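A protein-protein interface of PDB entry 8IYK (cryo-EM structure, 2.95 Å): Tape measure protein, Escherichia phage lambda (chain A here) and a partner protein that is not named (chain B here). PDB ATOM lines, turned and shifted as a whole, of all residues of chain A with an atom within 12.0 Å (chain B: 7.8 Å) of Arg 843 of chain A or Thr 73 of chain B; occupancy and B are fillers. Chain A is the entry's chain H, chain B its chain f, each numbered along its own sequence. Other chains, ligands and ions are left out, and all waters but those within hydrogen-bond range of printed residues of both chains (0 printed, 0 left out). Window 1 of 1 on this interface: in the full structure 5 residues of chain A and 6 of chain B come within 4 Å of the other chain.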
ATOM      1  N   GLY A 833      23.779 -12.132  12.977  1.00  0.00           N
ATOM      2  CA  GLY A 833      23.001 -12.521  14.141  1.00  0.00           C
ATOM      3  C   GLY A 833      23.499 -13.808  14.769  1.00  0.00           C
ATOM      4  O   GLY A 833      23.528 -13.941  15.992  1.00  0.00           O
ATOM      5  N   ALA A 834      23.895 -14.774  13.937  1.00  0.00           N
ATOM      6  CA  ALA A 834      24.440 -16.021  14.456  1.00  0.00           C
ATOM      7  C   ALA A 834      25.743 -15.784  15.204  1.00  0.00           C
ATOM      8  O   ALA A 834      25.962 -16.353  16.278  1.00  0.00           O
ATOM      9  CB  ALA A 834      24.649 -17.015  13.316  1.00  0.00           C
ATOM     10  N   ARG A 835      26.621 -14.943  14.653  1.00  0.00           N
ATOM     11  CA  ARG A 835      27.866 -14.629  15.351  1.00  0.00           C
ATOM     12  C   ARG A 835      27.594 -13.930  16.676  1.00  0.00           C
ATOM     13  O   ARG A 835      28.224 -14.243  17.695  1.00  0.00           O
ATOM     14  CB  ARG A 835      28.765 -13.766  14.468  1.00  0.00           C
ATOM     15  CG  ARG A 835      30.175 -14.301  14.317  1.00  0.00           C
ATOM     16  CD  ARG A 835      30.768 -13.913  12.976  1.00  0.00           C
ATOM     17  NE  ARG A 835      30.157 -12.703  12.443  1.00  0.00           N
ATOM     18  CZ  ARG A 835      29.756 -12.557  11.187  1.00  0.00           C
ATOM     19  NH1 ARG A 835      29.887 -13.532  10.304  1.00  0.00           N
ATOM     20  NH2 ARG A 835      29.211 -11.405  10.811  1.00  0.00           N
ATOM     21  N   ASP A 836      26.657 -12.979  16.684  1.00  0.00           N
ATOM     22  CA  ASP A 836      26.323 -12.276  17.918  1.00  0.00           C
ATOM     23  C   ASP A 836      25.749 -13.229  18.959  1.00  0.00           C
ATOM     24  O   ASP A 836      26.110 -13.161  20.138  1.00  0.00           O
ATOM     25  CB  ASP A 836      25.335 -11.149  17.627  1.00  0.00           C
ATOM     26  CG  ASP A 836      26.014  -9.905  17.096  1.00  0.00           C
ATOM     27  OD1 ASP A 836      27.074 -10.036  16.450  1.00  0.00           O
ATOM     28  OD2 ASP A 836      25.484  -8.799  17.323  1.00  0.00           O
ATOM     29  N   GLU A 837      24.858 -14.129  18.539  1.00  0.00           N
ATOM     30  CA  GLU A 837      24.276 -15.087  19.472  1.00  0.00           C
ATOM     31  C   GLU A 837      25.333 -16.038  20.016  1.00  0.00           C
ATOM     32  O   GLU A 837      25.327 -16.369  21.207  1.00  0.00           O
ATOM     33  CB  GLU A 837      23.153 -15.862  18.790  1.00  0.00           C
ATOM     34  CG  GLU A 837      22.308 -16.687  19.738  1.00  0.00           C
ATOM     35  CD  GLU A 837      21.254 -15.857  20.443  1.00  0.00           C
ATOM     36  OE1 GLU A 837      21.597 -15.166  21.425  1.00  0.00           O
ATOM     37  OE2 GLU A 837      20.084 -15.890  20.011  1.00  0.00           O
ATOM     38  N   ILE A 838      26.249 -16.492  19.158  1.00  0.00           N
ATOM     39  CA  ILE A 838      27.318 -17.373  19.615  1.00  0.00           C
ATOM     40  C   ILE A 838      28.176 -16.664  20.653  1.00  0.00           C
ATOM     41  O   ILE A 838      28.459 -17.210  21.724  1.00  0.00           O
ATOM     42  CB  ILE A 838      28.162 -17.861  18.424  1.00  0.00           C
ATOM     43  CG1 ILE A 838      27.410 -18.941  17.645  1.00  0.00           C
ATOM     44  CG2 ILE A 838      29.502 -18.389  18.902  1.00  0.00           C
ATOM     45  CD1 ILE A 838      27.979 -19.210  16.270  1.00  0.00           C
ATOM     46  N   GLN A 839      28.584 -15.426  20.362  1.00  0.00           N
ATOM     47  CA  GLN A 839      29.397 -14.681  21.319  1.00  0.00           C
ATOM     48  C   GLN A 839      28.634 -14.400  22.605  1.00  0.00           C
ATOM     49  O   GLN A 839      29.241 -14.299  23.677  1.00  0.00           O
ATOM     50  CB  GLN A 839      29.889 -13.378  20.692  1.00  0.00           C
ATOM     51  CG  GLN A 839      31.216 -13.510  19.966  1.00  0.00           C
ATOM     52  CD  GLN A 839      31.483 -12.353  19.026  1.00  0.00           C
ATOM     53  OE1 GLN A 839      30.647 -11.465  18.862  1.00  0.00           O
ATOM     54  NE2 GLN A 839      32.654 -12.358  18.400  1.00  0.00           N
ATOM     55  N   THR A 840      27.310 -14.266  22.522  1.00  0.00           N
ATOM     56  CA  THR A 840      26.508 -14.060  23.723  1.00  0.00           C
ATOM     57  C   THR A 840      26.459 -15.320  24.579  1.00  0.00           C
ATOM     58  O   THR A 840      26.541 -15.243  25.810  1.00  0.00           O
ATOM     59  CB  THR A 840      25.097 -13.615  23.337  1.00  0.00           C
ATOM     60  OG1 THR A 840      25.150 -12.306  22.759  1.00  0.00           O
ATOM     61  CG2 THR A 840      24.190 -13.585  24.553  1.00  0.00           C
ATOM     62  N   GLN A 841      26.337 -16.489  23.947  1.00  0.00           N
ATOM     63  CA  GLN A 841      26.238 -17.731  24.706  1.00  0.00           C
ATOM     64  C   GLN A 841      27.546 -18.115  25.386  1.00  0.00           C
ATOM     65  O   GLN A 841      27.523 -18.921  26.320  1.00  0.00           O
ATOM     66  CB  GLN A 841      25.771 -18.873  23.803  1.00  0.00           C
ATOM     67  CG  GLN A 841      24.405 -18.649  23.185  1.00  0.00           C
ATOM     68  CD  GLN A 841      23.350 -18.310  24.215  1.00  0.00           C
ATOM     69  OE1 GLN A 841      22.970 -19.149  25.029  1.00  0.00           O
ATOM     70  NE2 GLN A 841      22.870 -17.074  24.186  1.00  0.00           N
ATOM     71  N   MET A 842      28.678 -17.558  24.957  1.00  0.00           N
ATOM     72  CA  MET A 842      29.940 -17.808  25.645  1.00  0.00           C
ATOM     73  C   MET A 842      30.065 -17.037  26.950  1.00  0.00           C
ATOM     74  O   MET A 842      31.120 -17.102  27.590  1.00  0.00           O
ATOM     75  CB  MET A 842      31.129 -17.471  24.743  1.00  0.00           C
ATOM     76  CG  MET A 842      30.990 -17.939  23.310  1.00  0.00           C
ATOM     77  SD  MET A 842      32.063 -19.335  22.934  1.00  0.00           S
ATOM     78  CE  MET A 842      33.660 -18.531  22.903  1.00  0.00           C
ATOM     79  N   ARG A 843      29.027 -16.314  27.358  1.00  0.00           N
ATOM     80  CA  ARG A 843      29.027 -15.619  28.636  1.00  0.00           C
ATOM     81  C   ARG A 843      28.709 -16.618  29.746  1.00  0.00           C
ATOM     82  O   ARG A 843      28.729 -17.835  29.547  1.00  0.00           O
ATOM     83  CB  ARG A 843      28.053 -14.445  28.602  1.00  0.00           C
ATOM     84  CG  ARG A 843      28.613 -13.216  27.908  1.00  0.00           C
ATOM     85  CD  ARG A 843      27.907 -11.946  28.346  1.00  0.00           C
ATOM     86  NE  ARG A 843      26.859 -11.556  27.411  1.00  0.00           N
ATOM     87  CZ  ARG A 843      25.652 -11.142  27.769  1.00  0.00           C
ATOM     88  NH1 ARG A 843      25.304 -11.045  29.042  1.00  0.00           N
ATOM     89  NH2 ARG A 843      24.772 -10.818  26.827  1.00  0.00           N
ATOM     90  N   ASP A 844      28.415 -16.106  30.940  1.00  0.00           N
ATOM     91  CA  ASP A 844      28.346 -16.936  32.136  1.00  0.00           C
ATOM     92  C   ASP A 844      27.285 -18.026  32.060  1.00  0.00           C
ATOM     93  O   ASP A 844      27.619 -19.215  32.035  1.00  0.00           O
ATOM     94  CB  ASP A 844      28.075 -16.062  33.355  1.00  0.00           C
ATOM     95  CG  ASP A 844      29.271 -15.951  34.255  1.00  0.00           C
ATOM     96  OD1 ASP A 844      29.314 -14.982  35.034  1.00  0.00           O
ATOM     97  OD2 ASP A 844      30.166 -16.817  34.178  1.00  0.00           O
ATOM     98  N   GLY A 845      26.012 -17.644  32.029  1.00  0.00           N
ATOM     99  CA  GLY A 845      24.973 -18.651  31.991  1.00  0.00           C
ATOM    100  C   GLY A 845      24.891 -19.321  30.638  1.00  0.00           C
ATOM    101  O   GLY A 845      25.399 -20.431  30.463  1.00  0.00           O
ATOM    102  N   GLY A 846      24.276 -18.638  29.674  1.00  0.00           N
ATOM    103  CA  GLY A 846      24.324 -19.016  28.275  1.00  0.00           C
ATOM    104  C   GLY A 846      24.128 -20.484  27.964  1.00  0.00           C
ATOM    105  O   GLY A 846      23.421 -21.207  28.671  1.00  0.00           O
ATOM    106  N   LEU A 847      24.754 -20.921  26.874  1.00  0.00           N
ATOM    107  CA  LEU A 847      24.900 -22.328  26.552  1.00  0.00           C
ATOM    108  C   LEU A 847      26.341 -22.682  26.226  1.00  0.00           C
ATOM    109  O   LEU A 847      26.629 -23.854  25.960  1.00  0.00           O
ATOM    110  CB  LEU A 847      24.004 -22.709  25.365  1.00  0.00           C
ATOM    111  CG  LEU A 847      22.543 -23.042  25.663  1.00  0.00           C
ATOM    112  CD1 LEU A 847      21.664 -22.661  24.483  1.00  0.00           C
ATOM    113  CD2 LEU A 847      22.388 -24.515  25.997  1.00  0.00           C
ATOM    114  N   PHE A 848      27.248 -21.702  26.239  1.00  0.00           N
ATOM    115  CA  PHE A 848      28.611 -21.848  25.730  1.00  0.00           C
ATOM    116  C   PHE A 848      28.613 -22.304  24.276  1.00  0.00           C
ATOM    117  O   PHE A 848      29.547 -22.971  23.826  1.00  0.00           O
ATOM    118  CB  PHE A 848      29.448 -22.786  26.604  1.00  0.00           C
ATOM    119  CG  PHE A 848      29.907 -22.161  27.892  1.00  0.00           C
ATOM    120  CD1 PHE A 848      28.995 -21.624  28.786  1.00  0.00           C
ATOM    121  CD2 PHE A 848      31.254 -22.098  28.202  1.00  0.00           C
ATOM    122  CE1 PHE A 848      29.415 -21.044  29.965  1.00  0.00           C
ATOM    123  CE2 PHE A 848      31.681 -21.519  29.382  1.00  0.00           C
ATOM    124  CZ  PHE A 848      30.758 -20.992  30.262  1.00  0.00           C
ATOM    125  N   SER A 849      27.572 -21.916  23.543  1.00  0.00           N
ATOM    126  CA  SER A 849      27.409 -22.222  22.125  1.00  0.00           C
ATOM    127  C   SER A 849      27.726 -23.675  21.795  1.00  0.00           C
ATOM    128  O   SER A 849      27.083 -24.589  22.309  1.00  0.00           O
ATOM    129  CB  SER A 849      28.277 -21.287  21.282  1.00  0.00           C
ATOM    130  OG  SER A 849      29.639 -21.359  21.666  1.00  0.00           O
ATOM    131  N   GLU B  67      15.020  -5.995  31.234  1.00  0.00           N
ATOM    132  CA  GLU B  67      14.224  -7.162  31.578  1.00  0.00           C
ATOM    133  C   GLU B  67      14.786  -7.775  32.849  1.00  0.00           C
ATOM    134  O   GLU B  67      15.918  -7.494  33.247  1.00  0.00           O
ATOM    135  CB  GLU B  67      14.214  -8.189  30.443  1.00  0.00           C
ATOM    136  CG  GLU B  67      15.552  -8.350  29.750  1.00  0.00           C
ATOM    137  CD  GLU B  67      15.654  -9.647  28.976  1.00  0.00           C
ATOM    138  OE1 GLU B  67      15.360 -10.712  29.556  1.00  0.00           O
ATOM    139  OE2 GLU B  67      16.028  -9.601  27.785  1.00  0.00           O
ATOM    140  N   ASN B  69      15.307 -11.470  34.118  1.00  0.00           N
ATOM    141  CA  ASN B  69      15.327 -12.907  33.891  1.00  0.00           C
ATOM    142  C   ASN B  69      16.462 -13.519  34.694  1.00  0.00           C
ATOM    143  O   ASN B  69      17.612 -13.087  34.574  1.00  0.00           O
ATOM    144  CB  ASN B  69      15.496 -13.232  32.404  1.00  0.00           C
ATOM    145  CG  ASN B  69      15.185 -14.678  32.085  1.00  0.00           C
ATOM    146  OD1 ASN B  69      14.860 -15.466  32.971  1.00  0.00           O
ATOM    147  ND2 ASN B  69      15.289 -15.037  30.812  1.00  0.00           N
ATOM    148  N   GLY B  70      16.140 -14.522  35.505  1.00  0.00           N
ATOM    149  CA  GLY B  70      17.145 -15.188  36.309  1.00  0.00           C
ATOM    150  C   GLY B  70      17.862 -16.301  35.576  1.00  0.00           C
ATOM    151  O   GLY B  70      19.051 -16.543  35.806  1.00  0.00           O
ATOM    152  N   LYS B  71      17.148 -16.986  34.690  1.00  0.00           N
ATOM    153  CA  LYS B  71      17.716 -18.105  33.954  1.00  0.00           C
ATOM    154  C   LYS B  71      18.543 -17.612  32.773  1.00  0.00           C
ATOM    155  O   LYS B  71      18.143 -16.689  32.059  1.00  0.00           O
ATOM    156  CB  LYS B  71      16.607 -19.035  33.463  1.00  0.00           C
ATOM    157  CG  LYS B  71      17.015 -20.490  33.351  1.00  0.00           C
ATOM    158  CD  LYS B  71      15.921 -21.317  32.704  1.00  0.00           C
ATOM    159  CE  LYS B  71      16.254 -21.640  31.262  1.00  0.00           C
ATOM    160  NZ  LYS B  71      17.339 -22.649  31.162  1.00  0.00           N
ATOM    161  N   GLY B  72      19.695 -18.236  32.571  1.00  0.00           N
ATOM    162  CA  GLY B  72      20.542 -17.910  31.443  1.00  0.00           C
ATOM    163  C   GLY B  72      21.503 -16.773  31.734  1.00  0.00           C
ATOM    164  O   GLY B  72      21.880 -16.501  32.878  1.00  0.00           O
ATOM    165  N   THR B  73      21.908 -16.102  30.660  1.00  0.00           N
ATOM    166  CA  THR B  73      22.853 -15.002  30.767  1.00  0.00           C
ATOM    167  C   THR B  73      22.248 -13.834  31.538  1.00  0.00           C
ATOM    168  O   THR B  73      21.038 -13.599  31.508  1.00  0.00           O
ATOM    169  CB  THR B  73      23.286 -14.526  29.380  1.00  0.00           C
ATOM    170  OG1 THR B  73      22.156 -14.525  28.500  1.00  0.00           O
ATOM    171  CG2 THR B  73      24.363 -15.429  28.813  1.00  0.00           C
ATOM    172  N   SER B  74      23.110 -13.107  32.241  1.00  0.00           N
ATOM    173  CA  SER B  74      22.687 -11.882  32.901  1.00  0.00           C
ATOM    174  C   SER B  74      22.284 -10.845  31.861  1.00  0.00           C
ATOM    175  O   SER B  74      22.940 -10.693  30.828  1.00  0.00           O
ATOM    176  CB  SER B  74      23.811 -11.341  33.783  1.00  0.00           C
ATOM    177  OG  SER B  74      23.356 -10.273  34.589  1.00  0.00           O
ATOM    178  N   THR B  75      21.195 -10.133  32.137  1.00  0.00           N
ATOM    179  CA  THR B  75      20.669  -9.176  31.174  1.00  0.00           C
ATOM    180  C   THR B  75      21.637  -8.016  30.981  1.00  0.00           C
ATOM    181  O   THR B  75      22.198  -7.485  31.943  1.00  0.00           O
ATOM    182  CB  THR B  75      19.311  -8.651  31.636  1.00  0.00           C
ATOM    183  OG1 THR B  75      19.437  -8.092  32.948  1.00  0.00           O
ATOM    184  CG2 THR B  75      18.294  -9.779  31.670  1.00  0.00           C
ATOM    185  N   ARG B  76      21.830  -7.624  29.721  1.00  0.00           N
ATOM    186  CA  ARG B  76      22.734  -6.537  29.348  1.00  0.00           C
ATOM    187  C   ARG B  76      21.955  -5.503  28.547  1.00  0.00           C
ATOM    188  O   ARG B  76      21.851  -5.610  27.315  1.00  0.00           O
ATOM    189  CB  ARG B  76      23.928  -7.059  28.553  1.00  0.00           C
ATOM    190  CG  ARG B  76      25.055  -7.596  29.412  1.00  0.00           C
ATOM    191  CD  ARG B  76      26.397  -7.449  28.718  1.00  0.00           C
ATOM    192  NE  ARG B  76      27.505  -7.785  29.604  1.00  0.00           N
ATOM    193  CZ  ARG B  76      28.702  -8.176  29.192  1.00  0.00           C
ATOM    194  NH1 ARG B  76      28.986  -8.292  27.906  1.00  0.00           N
ATOM    195  NH2 ARG B  76      29.639  -8.456  30.094  1.00  0.00           N
ATOM    196  N   PRO B  77      21.388  -4.489  29.200  1.00  0.00           N
ATOM    197  CA  PRO B  77      20.648  -3.458  28.461  1.00  0.00           C
ATOM    198  C   PRO B  77      21.554  -2.607  27.590  1.00  0.00           C
ATOM    199  O   PRO B  77      22.780  -2.735  27.644  1.00  0.00           O
ATOM    200  CB  PRO B  77      20.001  -2.620  29.573  1.00  0.00           C
ATOM    201  CG  PRO B  77      20.104  -3.444  30.811  1.00  0.00           C
ATOM    202  CD  PRO B  77      21.325  -4.282  30.653  1.00  0.00           C
ATOM    203  N   GLU B 138      29.356  -1.000  31.054  1.00  0.00           N
ATOM    204  CA  GLU B 138      30.332  -2.051  30.800  1.00  0.00           C
ATOM    205  C   GLU B 138      31.237  -1.739  29.617  1.00  0.00           C
ATOM    206  O   GLU B 138      32.438  -2.014  29.674  1.00  0.00           O
ATOM    207  CB  GLU B 138      29.611  -3.382  30.565  1.00  0.00           C
ATOM    208  CG  GLU B 138      30.463  -4.464  29.931  1.00  0.00           C
ATOM    209  CD  GLU B 138      31.360  -5.164  30.932  1.00  0.00           C
ATOM    210  OE1 GLU B 138      31.178  -4.947  32.149  1.00  0.00           O
ATOM    211  OE2 GLU B 138      32.245  -5.933  30.501  1.00  0.00           O
ATOM    212  N   VAL B 151      26.737  -0.303  26.572  1.00  0.00           N
ATOM    213  CA  VAL B 151      26.242  -1.564  27.106  1.00  0.00           C
ATOM    214  C   VAL B 151      26.152  -1.414  28.615  1.00  0.00           C
ATOM    215  O   VAL B 151      27.090  -0.929  29.257  1.00  0.00           O
ATOM    216  CB  VAL B 151      27.153  -2.738  26.718  1.00  0.00           C
ATOM    217  CG1 VAL B 151      26.400  -4.050  26.837  1.00  0.00           C
ATOM    218  CG2 VAL B 151      27.681  -2.556  25.310  1.00  0.00           C
ATOM    219  N   LEU B 152      25.017  -1.796  29.181  1.00  0.00           N
ATOM    220  CA  LEU B 152      24.832  -1.769  30.621  1.00  0.00           C
ATOM    221  C   LEU B 152      24.788  -3.187  31.167  1.00  0.00           C
ATOM    222  O   LEU B 152      24.519  -4.150  30.447  1.00  0.00           O
ATOM    223  CB  LEU B 152      23.556  -1.015  30.998  1.00  0.00           C
ATOM    224  CG  LEU B 152      23.384   0.365  30.369  1.00  0.00           C
ATOM    225  CD1 LEU B 152      22.124   1.028  30.888  1.00  0.00           C
ATOM    226  CD2 LEU B 152      24.598   1.228  30.651  1.00  0.00           C
ATOM    227  N   SER B 153      25.071  -3.306  32.459  1.00  0.00           N
ATOM    228  CA  SER B 153      25.103  -4.604  33.111  1.00  0.00           C
ATOM    229  C   SER B 153      24.637  -4.451  34.548  1.00  0.00           C
ATOM    230  O   SER B 153      24.708  -3.366  35.127  1.00  0.00           O
ATOM    231  CB  SER B 153      26.505  -5.219  33.069  1.00  0.00           C
ATOM    232  OG  SER B 153      27.343  -4.640  34.053  1.00  0.00           O
ATOM    233  N   THR B 154      24.144  -5.547  35.115  1.00  0.00           N
ATOM    234  CA  THR B 154      23.808  -5.540  36.525  1.00  0.00           C
ATOM    235  C   THR B 154      25.086  -5.393  37.350  1.00  0.00           C
ATOM    236  O   THR B 154      26.147  -5.886  36.958  1.00  0.00           O
ATOM    237  CB  THR B 154      23.069  -6.818  36.915  1.00  0.00           C
ATOM    238  OG1 THR B 154      23.989  -7.755  37.484  1.00  0.00           O
ATOM    239  CG2 THR B 154      22.406  -7.435  35.701  1.00  0.00           C
ATOM    240  N   GLU B 157      26.995  -9.291  38.178  1.00  0.00           N
ATOM    241  CA  GLU B 157      27.676  -9.719  36.955  1.00  0.00           C
ATOM    242  C   GLU B 157      28.927 -10.551  37.220  1.00  0.00           C
ATOM    243  O   GLU B 157      30.046 -10.084  36.991  1.00  0.00           O
ATOM    244  CB  GLU B 157      28.018  -8.512  36.083  1.00  0.00           C
ATOM    245  CG  GLU B 157      28.431  -8.894  34.671  1.00  0.00           C
ATOM    246  CD  GLU B 157      27.348  -8.634  33.649  1.00  0.00           C
ATOM    247  OE1 GLU B 157      26.165  -8.552  34.041  1.00  0.00           O
ATOM    248  OE2 GLU B 157      27.676  -8.518  32.450  1.00  0.00           O
ATOM    249  N   ASP B 159      31.074 -12.270  36.040  1.00  0.00           N
ATOM    250  CA  ASP B 159      31.573 -12.746  34.754  1.00  0.00           C
ATOM    251  C   ASP B 159      33.034 -13.177  34.833  1.00  0.00           C
ATOM    252  O   ASP B 159      33.358 -14.351  34.625  1.00  0.00           O
ATOM    253  CB  ASP B 159      31.395 -11.658  33.692  1.00  0.00           C
ATOM    254  CG  ASP B 159      30.726 -12.176  32.436  1.00  0.00           C
ATOM    255  OD1 ASP B 159      29.493 -12.375  32.455  1.00  0.00           O
ATOM    256  OD2 ASP B 159      31.431 -12.379  31.425  1.00  0.00           O
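The guanidinium group (NH1) of Arg 843 of chain A is in hydrogen-bond range of the backbone carbonyl oxygen (O) of Ser 74 of chain B.
The backbone NH (N) of Asp 159 of chain B lies close to the side-chain carboxylate (OD1) of Asp 844 of chain A (3.4 Å).
OG of Ser 74 of chain B sits at hydrogen-bond distance from OE1 of Glu 157 of chain B (3.3 Å).
NH2 of Arg 76 of chain B is in salt-bridge range of OE2 of Glu 138 of chain B (3.6 Å).
NE of Arg 76 of chain B is in salt-bridge range of OE2 of Glu 157 of chain B, at 2.9 Å.
OG1 of Thr 840 of chain A sits at hydrogen-bond distance from O of Asp 836 of chain A (2.9 Å).
Thr 840 of chain A touches Thr 73 of chain B.
Arg 843 of chain A touches Thr 73 of chain B.
Arg 843 of chain A touches Arg 76 of chain B (NH1 to CG, 3.5 Å).
Gly 845 of chain A touches Gly 72 of chain B.
Gly 846 of chain A touches Gly 72 of chain B.
Gly 846 of chain A touches Thr 73 of chain B.
Gln 839 of chain A touches none of the printed residues of chain B.
Arg 843 of chain A touches just these residues of chain B: Thr 73, Ser 74 and Arg 76.
Of the printed residues of chain B, Gly 845 of chain A touches Gly 72.
Printed residues of chain B within 4 Å of Gly 846 of chain A: Gly 72 and Thr 73.
Leu 847 of chain A touches none of the printed residues of chain B.
Asn 69 of chain B touches none of the printed residues of chain A.
Of chain A, only Gly 845 and Gly 846 come within 4 Å of Gly 72 of chain B.
Of chain A, only Thr 840 (3.7 Å), Arg 843 (3.8 Å) and Gly 846 (3.3 Å) come within 4 Å of Thr 73 of chain B.
Of chain A, only Arg 843 comes within 4 Å of Ser 74 of chain B.
Arg 76 of chain B touches one residue of chain A.
Of the printed residues of chain A, Asp 159 of chain B touches Asp 844.
Printed residues of chain B that touch a printed residue of chain A: Gly 72, Thr 73, Ser 74, Arg 76 and Asp 159.
Of the 17 printed residues of chain A, 5 touch a printed residue of chain B.
Printed residues of chain A that touch a printed residue of chain B: Thr 840, Arg 843, Asp 844, Gly 845 and Gly 846.
Along chain A the printed residues that touch a printed residue of chain B span positions 840 to 846.
Among the printed residues, 8 pairs touch across the chains.
Among the printed residues, no Asp or Glu carboxylate lies within 4 Å of a Lys or Arg side-chain nitrogen of the other chain.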
